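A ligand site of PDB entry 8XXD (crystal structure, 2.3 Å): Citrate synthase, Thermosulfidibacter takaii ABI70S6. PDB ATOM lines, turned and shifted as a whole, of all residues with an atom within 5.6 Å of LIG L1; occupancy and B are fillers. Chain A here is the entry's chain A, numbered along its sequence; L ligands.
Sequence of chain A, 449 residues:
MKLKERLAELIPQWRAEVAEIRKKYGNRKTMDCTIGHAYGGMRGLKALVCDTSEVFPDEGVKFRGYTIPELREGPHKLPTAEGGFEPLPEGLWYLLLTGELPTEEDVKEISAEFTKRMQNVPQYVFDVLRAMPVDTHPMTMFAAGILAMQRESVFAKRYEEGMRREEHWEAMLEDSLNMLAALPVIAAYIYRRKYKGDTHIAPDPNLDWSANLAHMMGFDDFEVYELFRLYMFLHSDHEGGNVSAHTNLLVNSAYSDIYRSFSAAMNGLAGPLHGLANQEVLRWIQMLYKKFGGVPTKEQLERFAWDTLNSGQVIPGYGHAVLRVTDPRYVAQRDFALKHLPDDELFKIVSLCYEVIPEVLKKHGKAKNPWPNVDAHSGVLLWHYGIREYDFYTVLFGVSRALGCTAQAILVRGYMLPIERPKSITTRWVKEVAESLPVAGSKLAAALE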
ATOM      1  N   ARG A  43       4.666   1.401 -28.910  1.00  0.00           N
ATOM      2  CA  ARG A  43       5.739   0.479 -29.285  1.00  0.00           C
ATOM      3  C   ARG A  43       5.815   0.370 -30.806  1.00  0.00           C
ATOM      4  O   ARG A  43       4.826   0.134 -31.470  1.00  0.00           O
ATOM      5  CB  ARG A  43       5.521  -0.925 -28.700  1.00  0.00           C
ATOM      6  CG  ARG A  43       6.781  -1.769 -28.580  1.00  0.00           C
ATOM      7  CD  ARG A  43       7.825  -1.197 -27.614  1.00  0.00           C
ATOM      8  NE  ARG A  43       7.190  -0.492 -26.497  1.00  0.00           N
ATOM      9  CZ  ARG A  43       7.041  -0.961 -25.256  1.00  0.00           C
ATOM     10  NH1 ARG A  43       7.908  -1.840 -24.763  1.00  0.00           N
ATOM     11  NH2 ARG A  43       6.060  -0.505 -24.495  1.00  0.00           N
ATOM     12  N   ALA A 277      17.374  -1.667 -13.708  1.00  0.00           N
ATOM     13  CA  ALA A 277      17.760  -2.992 -14.191  1.00  0.00           C
ATOM     14  C   ALA A 277      19.138  -3.469 -13.709  1.00  0.00           C
ATOM     15  O   ALA A 277      19.295  -4.628 -13.313  1.00  0.00           O
ATOM     16  CB  ALA A 277      17.711  -2.974 -15.695  1.00  0.00           C
ATOM     17  N   GLU A 280      18.841  -4.874 -10.117  1.00  0.00           N
ATOM     18  CA  GLU A 280      18.152  -6.150 -10.083  1.00  0.00           C
ATOM     19  C   GLU A 280      19.116  -7.265 -10.489  1.00  0.00           C
ATOM     20  O   GLU A 280      19.174  -8.298  -9.827  1.00  0.00           O
ATOM     21  CB  GLU A 280      16.965  -6.206 -11.059  1.00  0.00           C
ATOM     22  CG  GLU A 280      15.811  -5.271 -10.740  1.00  0.00           C
ATOM     23  CD  GLU A 280      14.784  -5.190 -11.865  1.00  0.00           C
ATOM     24  OE1 GLU A 280      13.945  -4.239 -11.844  1.00  0.00           O
ATOM     25  OE2 GLU A 280      14.813  -6.074 -12.778  1.00  0.00           O
ATOM     26  N   VAL A 281      19.848  -7.055 -11.590  1.00  0.00           N
ATOM     27  CA  VAL A 281      20.777  -8.070 -12.046  1.00  0.00           C
ATOM     28  C   VAL A 281      21.786  -8.369 -10.925  1.00  0.00           C
ATOM     29  O   VAL A 281      21.943  -9.530 -10.512  1.00  0.00           O
ATOM     30  CB  VAL A 281      21.427  -7.697 -13.399  1.00  0.00           C
ATOM     31  CG1 VAL A 281      22.599  -8.600 -13.792  1.00  0.00           C
ATOM     32  CG2 VAL A 281      20.403  -7.695 -14.530  1.00  0.00           C
ATOM     33  N   LEU A 309      11.944 -19.461 -15.017  1.00  0.00           N
ATOM     34  CA  LEU A 309      11.055 -19.238 -16.151  1.00  0.00           C
ATOM     35  C   LEU A 309       9.681 -19.885 -15.913  1.00  0.00           C
ATOM     36  O   LEU A 309       8.662 -19.218 -16.016  1.00  0.00           O
ATOM     37  CB  LEU A 309      11.731 -19.788 -17.402  1.00  0.00           C
ATOM     38  CG  LEU A 309      12.830 -18.875 -17.945  1.00  0.00           C
ATOM     39  CD1 LEU A 309      13.592 -19.535 -19.095  1.00  0.00           C
ATOM     40  CD2 LEU A 309      12.217 -17.557 -18.385  1.00  0.00           C
ATOM     41  N   GLN A 313       8.726 -16.049 -13.754  1.00  0.00           N
ATOM     42  CA  GLN A 313       9.597 -14.978 -13.315  1.00  0.00           C
ATOM     43  C   GLN A 313      10.439 -14.524 -14.503  1.00  0.00           C
ATOM     44  O   GLN A 313      10.610 -15.254 -15.482  1.00  0.00           O
ATOM     45  CB  GLN A 313      10.471 -15.431 -12.140  1.00  0.00           C
ATOM     46  CG  GLN A 313       9.694 -15.790 -10.882  1.00  0.00           C
ATOM     47  CD  GLN A 313       9.186 -14.588 -10.106  1.00  0.00           C
ATOM     48  OE1 GLN A 313       9.798 -14.177  -9.134  1.00  0.00           O
ATOM     49  NE2 GLN A 313       8.062 -14.020 -10.544  1.00  0.00           N
ATOM     50  N   VAL A 314      10.959 -13.290 -14.388  1.00  0.00           N
ATOM     51  CA  VAL A 314      11.869 -12.703 -15.358  1.00  0.00           C
ATOM     52  C   VAL A 314      13.317 -13.106 -15.017  1.00  0.00           C
ATOM     53  O   VAL A 314      13.682 -13.090 -13.846  1.00  0.00           O
ATOM     54  CB  VAL A 314      11.694 -11.167 -15.424  1.00  0.00           C
ATOM     55  CG1 VAL A 314      10.305 -10.801 -15.932  1.00  0.00           C
ATOM     56  CG2 VAL A 314      11.976 -10.462 -14.095  1.00  0.00           C
ATOM     57  N   ILE A 315      14.104 -13.514 -16.038  1.00  0.00           N
ATOM     58  CA  ILE A 315      15.557 -13.587 -15.915  1.00  0.00           C
ATOM     59  C   ILE A 315      16.161 -12.212 -16.195  1.00  0.00           C
ATOM     60  O   ILE A 315      16.331 -11.829 -17.362  1.00  0.00           O
ATOM     61  CB  ILE A 315      16.163 -14.636 -16.872  1.00  0.00           C
ATOM     62  CG1 ILE A 315      15.820 -16.064 -16.449  1.00  0.00           C
ATOM     63  CG2 ILE A 315      17.677 -14.437 -16.955  1.00  0.00           C
ATOM     64  CD1 ILE A 315      16.481 -17.120 -17.309  1.00  0.00           C
ATOM     65  N   PRO A 316      16.611 -11.438 -15.170  1.00  0.00           N
ATOM     66  CA  PRO A 316      16.972 -10.043 -15.376  1.00  0.00           C
ATOM     67  C   PRO A 316      18.266  -9.978 -16.207  1.00  0.00           C
ATOM     68  O   PRO A 316      19.156 -10.791 -16.056  1.00  0.00           O
ATOM     69  CB  PRO A 316      17.138  -9.445 -13.972  1.00  0.00           C
ATOM     70  CG  PRO A 316      16.875 -10.588 -12.990  1.00  0.00           C
ATOM     71  CD  PRO A 316      16.925 -11.874 -13.795  1.00  0.00           C
ATOM     72  N   GLY A 317      18.304  -9.028 -17.137  1.00  0.00           N
ATOM     73  CA  GLY A 317      19.501  -8.695 -17.888  1.00  0.00           C
ATOM     74  C   GLY A 317      19.460  -9.205 -19.310  1.00  0.00           C
ATOM     75  O   GLY A 317      20.351  -8.879 -20.098  1.00  0.00           O
ATOM     76  N   TYR A 318      18.437 -10.028 -19.613  1.00  0.00           N
ATOM     77  CA  TYR A 318      18.235 -10.650 -20.914  1.00  0.00           C
ATOM     78  C   TYR A 318      16.901 -10.198 -21.520  1.00  0.00           C
ATOM     79  O   TYR A 318      15.939  -9.941 -20.797  1.00  0.00           O
ATOM     80  CB  TYR A 318      18.366 -12.161 -20.741  1.00  0.00           C
ATOM     81  CG  TYR A 318      19.782 -12.612 -20.472  1.00  0.00           C
ATOM     82  CD1 TYR A 318      20.399 -12.399 -19.249  1.00  0.00           C
ATOM     83  CD2 TYR A 318      20.521 -13.246 -21.458  1.00  0.00           C
ATOM     84  CE1 TYR A 318      21.712 -12.807 -19.016  1.00  0.00           C
ATOM     85  CE2 TYR A 318      21.831 -13.645 -21.253  1.00  0.00           C
ATOM     86  CZ  TYR A 318      22.432 -13.430 -20.024  1.00  0.00           C
ATOM     87  OH  TYR A 318      23.718 -13.880 -19.869  1.00  0.00           O
ATOM     88  N   GLY A 319      16.881 -10.025 -22.850  1.00  0.00           N
ATOM     89  CA  GLY A 319      15.734  -9.464 -23.543  1.00  0.00           C
ATOM     90  C   GLY A 319      15.692  -7.937 -23.501  1.00  0.00           C
ATOM     91  O   GLY A 319      16.080  -7.318 -22.510  1.00  0.00           O
ATOM     92  N   HIS A 320      15.149  -7.329 -24.553  1.00  0.00           N
ATOM     93  CA  HIS A 320      14.997  -5.880 -24.637  1.00  0.00           C
ATOM     94  C   HIS A 320      13.708  -5.556 -25.392  1.00  0.00           C
ATOM     95  O   HIS A 320      13.178  -6.408 -26.121  1.00  0.00           O
ATOM     96  CB  HIS A 320      16.218  -5.254 -25.337  1.00  0.00           C
ATOM     97  CG  HIS A 320      16.407  -3.785 -25.130  1.00  0.00           C
ATOM     98  ND1 HIS A 320      16.272  -2.860 -26.152  1.00  0.00           N
ATOM     99  CD2 HIS A 320      16.734  -3.067 -24.043  1.00  0.00           C
ATOM    100  CE1 HIS A 320      16.495  -1.636 -25.674  1.00  0.00           C
ATOM    101  NE2 HIS A 320      16.794  -1.735 -24.394  1.00  0.00           N
ATOM    102  N   ALA A 321      13.245  -4.305 -25.244  1.00  0.00           N
ATOM    103  CA  ALA A 321      12.077  -3.785 -25.934  1.00  0.00           C
ATOM    104  C   ALA A 321      12.353  -3.385 -27.396  1.00  0.00           C
ATOM    105  O   ALA A 321      11.432  -2.867 -28.038  1.00  0.00           O
ATOM    106  CB  ALA A 321      11.539  -2.602 -25.153  1.00  0.00           C
ATOM    107  N   ARG A 324      17.815  -7.160 -30.486  1.00  0.00           N
ATOM    108  CA  ARG A 324      17.414  -8.471 -30.974  1.00  0.00           C
ATOM    109  C   ARG A 324      18.576  -9.473 -30.981  1.00  0.00           C
ATOM    110  O   ARG A 324      18.307 -10.667 -30.934  1.00  0.00           O
ATOM    111  CB  ARG A 324      16.764  -8.306 -32.347  1.00  0.00           C
ATOM    112  CG  ARG A 324      15.489  -9.121 -32.581  1.00  0.00           C
ATOM    113  CD  ARG A 324      14.381  -9.072 -31.531  1.00  0.00           C
ATOM    114  NE  ARG A 324      14.174  -7.813 -30.806  1.00  0.00           N
ATOM    115  CZ  ARG A 324      13.078  -7.498 -30.106  1.00  0.00           C
ATOM    116  NH1 ARG A 324      13.179  -6.741 -29.019  1.00  0.00           N
ATOM    117  NH2 ARG A 324      11.912  -8.050 -30.385  1.00  0.00           N
ATOM    118  N   LEU A 361      16.500 -19.559 -23.078  1.00  0.00           N
ATOM    119  CA  LEU A 361      15.446 -18.565 -23.305  1.00  0.00           C
ATOM    120  C   LEU A 361      14.863 -18.689 -24.719  1.00  0.00           C
ATOM    121  O   LEU A 361      13.736 -18.230 -24.945  1.00  0.00           O
ATOM    122  CB  LEU A 361      16.017 -17.154 -23.061  1.00  0.00           C
ATOM    123  CG  LEU A 361      15.855 -16.586 -21.649  1.00  0.00           C
ATOM    124  CD1 LEU A 361      16.732 -15.362 -21.453  1.00  0.00           C
ATOM    125  CD2 LEU A 361      14.397 -16.223 -21.356  1.00  0.00           C
ATOM    126  N   HIS A 364      12.208 -21.678 -24.218  1.00  0.00           N
ATOM    127  CA  HIS A 364      11.052 -21.157 -23.507  1.00  0.00           C
ATOM    128  C   HIS A 364      10.155 -20.314 -24.431  1.00  0.00           C
ATOM    129  O   HIS A 364       8.936 -20.342 -24.293  1.00  0.00           O
ATOM    130  CB  HIS A 364      11.483 -20.384 -22.255  1.00  0.00           C
ATOM    131  CG  HIS A 364      10.346 -19.859 -21.428  1.00  0.00           C
ATOM    132  ND1 HIS A 364      10.159 -18.503 -21.178  1.00  0.00           N
ATOM    133  CD2 HIS A 364       9.345 -20.491 -20.784  1.00  0.00           C
ATOM    134  CE1 HIS A 364       9.093 -18.346 -20.397  1.00  0.00           C
ATOM    135  NE2 HIS A 364       8.578 -19.536 -20.150  1.00  0.00           N
ATOM    136  N   LYS A 366       9.172 -17.224 -25.044  1.00  0.00           N
ATOM    137  CA  LYS A 366       8.346 -16.051 -24.757  1.00  0.00           C
ATOM    138  C   LYS A 366       9.135 -14.779 -25.066  1.00  0.00           C
ATOM    139  O   LYS A 366       8.602 -13.863 -25.683  1.00  0.00           O
ATOM    140  CB  LYS A 366       7.820 -16.058 -23.319  1.00  0.00           C
ATOM    141  CG  LYS A 366       6.972 -17.269 -22.982  1.00  0.00           C
ATOM    142  CD  LYS A 366       6.015 -17.095 -21.820  1.00  0.00           C
ATOM    143  CE  LYS A 366       5.388 -18.405 -21.418  1.00  0.00           C
ATOM    144  NZ  LYS A 366       4.271 -18.227 -20.467  1.00  0.00           N
ATOM    145  N   ALA A 367      10.409 -14.742 -24.636  1.00  0.00           N
ATOM    146  CA  ALA A 367      11.303 -13.621 -24.900  1.00  0.00           C
ATOM    147  C   ALA A 367      11.513 -13.438 -26.406  1.00  0.00           C
ATOM    148  O   ALA A 367      11.877 -14.388 -27.109  1.00  0.00           O
ATOM    149  CB  ALA A 367      12.621 -13.817 -24.175  1.00  0.00           C
ATOM    150  N   LYS A 368      11.301 -12.203 -26.882  1.00  0.00           N
ATOM    151  CA  LYS A 368      11.554 -11.842 -28.266  1.00  0.00           C
ATOM    152  C   LYS A 368      13.078 -11.712 -28.487  1.00  0.00           C
ATOM    153  O   LYS A 368      13.570 -12.114 -29.538  1.00  0.00           O
ATOM    154  CB  LYS A 368      10.743 -10.587 -28.627  1.00  0.00           C
ATOM    155  N   ASN A 369      13.806 -11.181 -27.478  1.00  0.00           N
ATOM    156  CA  ASN A 369      15.287 -11.117 -27.507  1.00  0.00           C
ATOM    157  C   ASN A 369      15.894 -12.080 -26.472  1.00  0.00           C
ATOM    158  O   ASN A 369      15.782 -11.844 -25.265  1.00  0.00           O
ATOM    159  CB  ASN A 369      15.813  -9.694 -27.268  1.00  0.00           C
ATOM    160  CG  ASN A 369      17.331  -9.597 -27.236  1.00  0.00           C
ATOM    161  OD1 ASN A 369      18.033 -10.444 -27.786  1.00  0.00           O
ATOM    162  ND2 ASN A 369      17.850  -8.558 -26.609  1.00  0.00           N
ATOM    163  N   ASN A 373      21.356  -7.608 -22.431  1.00  0.00           N
ATOM    164  CA  ASN A 373      21.494  -6.162 -22.601  1.00  0.00           C
ATOM    165  C   ASN A 373      22.644  -5.653 -21.716  1.00  0.00           C
ATOM    166  O   ASN A 373      23.413  -6.453 -21.186  1.00  0.00           O
ATOM    167  CB  ASN A 373      20.176  -5.450 -22.307  1.00  0.00           C
ATOM    168  CG  ASN A 373      19.702  -5.613 -20.876  1.00  0.00           C
ATOM    169  OD1 ASN A 373      20.467  -5.387 -19.938  1.00  0.00           O
ATOM    170  ND2 ASN A 373      18.446  -5.997 -20.696  1.00  0.00           N
ATOM    171  N   ASP A 375      22.645  -3.976 -18.867  1.00  0.00           N
ATOM    172  CA  ASP A 375      22.439  -4.061 -17.434  1.00  0.00           C
ATOM    173  C   ASP A 375      22.811  -5.433 -16.884  1.00  0.00           C
ATOM    174  O   ASP A 375      22.996  -5.572 -15.664  1.00  0.00           O
ATOM    175  CB  ASP A 375      20.996  -3.677 -17.140  1.00  0.00           C
ATOM    176  CG  ASP A 375      20.681  -2.327 -17.762  1.00  0.00           C
ATOM    177  OD1 ASP A 375      21.407  -1.362 -17.422  1.00  0.00           O
ATOM    178  OD2 ASP A 375      19.768  -2.271 -18.631  1.00  0.00           O
HETATM  179  N1  LIG L   1      12.413 -13.744 -18.538  1.00  0.00           N
HETATM  180  C1  LIG L   1      11.125 -14.096 -18.644  1.00  0.00           C
HETATM  181  N2  LIG L   1      10.221 -13.746 -19.548  1.00  0.00           N
HETATM  182  C2  LIG L   1      10.757 -12.908 -20.465  1.00  0.00           C
HETATM  183  C3  LIG L   1      12.057 -12.454 -20.496  1.00  0.00           C
HETATM  184  C4  LIG L   1      12.924 -12.902 -19.472  1.00  0.00           C
HETATM  185  N3  LIG L   1      14.200 -12.539 -19.399  1.00  0.00           N
HETATM  186  N4  LIG L   1      12.253 -11.610 -21.576  1.00  0.00           N
HETATM  187  C5  LIG L   1      11.083 -11.561 -22.174  1.00  0.00           C
HETATM  188  N5  LIG L   1      10.124 -12.339 -21.536  1.00  0.00           N
HETATM  189  C6  LIG L   1       8.712 -12.522 -21.923  1.00  0.00           C
HETATM  190  C7  LIG L   1       7.782 -11.381 -21.527  1.00  0.00           C
HETATM  191  O1  LIG L   1       7.487 -11.438 -20.154  1.00  0.00           O
HETATM  192  C8  LIG L   1       6.592 -11.640 -22.455  1.00  0.00           C
HETATM  193  O2  LIG L   1       5.670 -12.585 -21.929  1.00  0.00           O
HETATM  194  P1  LIG L   1       4.215 -11.986 -21.549  1.00  0.00           P
HETATM  195  O3  LIG L   1       4.346 -10.634 -20.834  1.00  0.00           O
HETATM  196  O4  LIG L   1       3.653 -13.064 -20.632  1.00  0.00           O
HETATM  197  O5  LIG L   1       3.403 -11.846 -22.835  1.00  0.00           O
HETATM  198  C9  LIG L   1       7.252 -12.188 -23.717  1.00  0.00           C
HETATM  199  O6  LIG L   1       8.601 -12.562 -23.331  1.00  0.00           O
HETATM  200  C10 LIG L   1       7.294 -11.235 -24.884  1.00  0.00           C
HETATM  201  O7  LIG L   1       7.809  -9.954 -24.447  1.00  0.00           O
HETATM  202  P2  LIG L   1       9.046  -9.240 -25.204  1.00  0.00           P
HETATM  203  O8  LIG L   1       8.573  -8.588 -26.474  1.00  0.00           O
HETATM  204  O9  LIG L   1      10.171 -10.220 -25.348  1.00  0.00           O
HETATM  205  O10 LIG L   1       9.414  -8.143 -24.090  1.00  0.00           O
HETATM  206  P3  LIG L   1       8.833  -6.730 -23.551  1.00  0.00           P
HETATM  207  O11 LIG L   1       9.150  -5.689 -24.582  1.00  0.00           O
HETATM  208  O12 LIG L   1       7.434  -6.909 -23.040  1.00  0.00           O
HETATM  209  O13 LIG L   1       9.782  -6.463 -22.282  1.00  0.00           O
HETATM  210  C11 LIG L   1      11.912  -6.100 -21.151  1.00  0.00           C
HETATM  211  C12 LIG L   1      11.147  -5.976 -22.474  1.00  0.00           C
HETATM  212  C13 LIG L   1      13.287  -5.443 -21.336  1.00  0.00           C
HETATM  213  C14 LIG L   1      11.139  -5.341 -20.068  1.00  0.00           C
HETATM  214  C15 LIG L   1      12.070  -7.593 -20.763  1.00  0.00           C
HETATM  215  O14 LIG L   1      12.968  -8.256 -21.684  1.00  0.00           O
HETATM  216  C16 LIG L   1      12.492  -7.840 -19.306  1.00  0.00           C
HETATM  217  O15 LIG L   1      11.630  -7.869 -18.438  1.00  0.00           O
HETATM  218  N6  LIG L   1      13.789  -8.021 -19.049  1.00  0.00           N
HETATM  219  C17 LIG L   1      14.334  -8.278 -17.722  1.00  0.00           C
HETATM  220  C18 LIG L   1      14.757  -7.010 -16.971  1.00  0.00           C
HETATM  221  C19 LIG L   1      15.876  -6.259 -17.672  1.00  0.00           C
HETATM  222  O16 LIG L   1      16.945  -6.812 -17.921  1.00  0.00           O
HETATM  223  N7  LIG L   1      15.626  -4.980 -18.011  1.00  0.00           N
HETATM  224  C20 LIG L   1      16.586  -4.113 -18.683  1.00  0.00           C
HETATM  225  C21 LIG L   1      16.019  -3.392 -19.888  1.00  0.00           C
HETATM  226  S1  LIG L   1      17.124  -2.090 -20.494  1.00  0.00           S
HETATM  227  O1  LG2 L   2      16.501   2.058 -24.819  1.00  0.00           O
HETATM  228  O2  LG2 L   2      14.589   1.196 -24.162  1.00  0.00           O
HETATM  229  O3  LG2 L   2      19.772   2.535 -22.452  1.00  0.00           O
HETATM  230  O4  LG2 L   2      17.811   3.503 -22.372  1.00  0.00           O
HETATM  231  O5  LG2 L   2      18.534   0.277 -22.808  1.00  0.00           O
HETATM  232  C1  LG2 L   2      15.776   1.510 -23.970  1.00  0.00           C
HETATM  233  C2  LG2 L   2      16.384   1.214 -22.600  1.00  0.00           C
HETATM  234  C3  LG2 L   2      17.901   1.316 -22.621  1.00  0.00           C
HETATM  235  C4  LG2 L   2      18.510   2.487 -22.471  1.00  0.00           C
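O of Lys 366 sits close to O6 of LIG L1, at 2.7 Å.
O of Gly 319 lies close to O14 of LIG L1, 3.4 Å away.
OD2 of Asp 375 sits close to S1 of LIG L1, 3.2 Å away.
O of Tyr 318 sits at hydrogen-bond distance from N6 of LIG L1.
An oxygen (O9) of LIG L1 lies within hydrogen-bond range of the backbone NH of Lys 368, 2.7 Å away.
An oxygen (O5) of LG2 L2 lies within hydrogen-bond range of a ring nitrogen (NE2) of His 320 (3.1 Å).
O of Ile 315 lies within hydrogen-bond range of N3 of LIG L1, at 3.0 Å.
The side-chain amide nitrogen (ND2) of Asn 373 lies within hydrogen-bond range of an oxygen (O16) of LIG L1, 3.3 Å away.
The backbone NH (N) of Ile 315 is in hydrogen-bond range of a nitrogen (N1) of LIG L1 (3.0 Å).
N of Gly 317 is in hydrogen-bond range of O16 of LIG L1.
O6 of LIG L1 lies within hydrogen-bond range of N of Ala 367.
An oxygen (O5) of LG2 L2 lies close to a sulfur (S1) of LIG L1, at 3.6 Å.
The backbone NH (N) of Asp 375 is in hydrogen-bond range of the side-chain amide oxygen (OD1) of Asn 373, at 2.8 Å.
The side-chain amide nitrogen (ND2) of Asn 373 lies within hydrogen-bond range of the backbone carbonyl oxygen (O) of Gly 319 (3.3 Å).
The backbone carbonyl oxygen of Gly 317 lies within hydrogen-bond range of the backbone NH of Asn 373 (2.8 Å).
NH1 of Arg 324 lies within hydrogen-bond range of O of His 320 (2.9 Å).
The backbone carbonyl oxygen (O) of Asn 369 lies close to the backbone NH (N) of Gly 319, at 3.2 Å.
Merely in contact with LIG L1: Ala 277, Val 314, Gln 313, Leu 309, His 320, Ala 321 and Pro 316.
Hydrophobic or aromatic side chains that line LIG L1: Ala 277, Leu 309, Ile 315, His 320, Ala 321 and Ala 367.
The nearest printed residue that does not touch LIG L1 is Arg 43 (4.05 Å).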
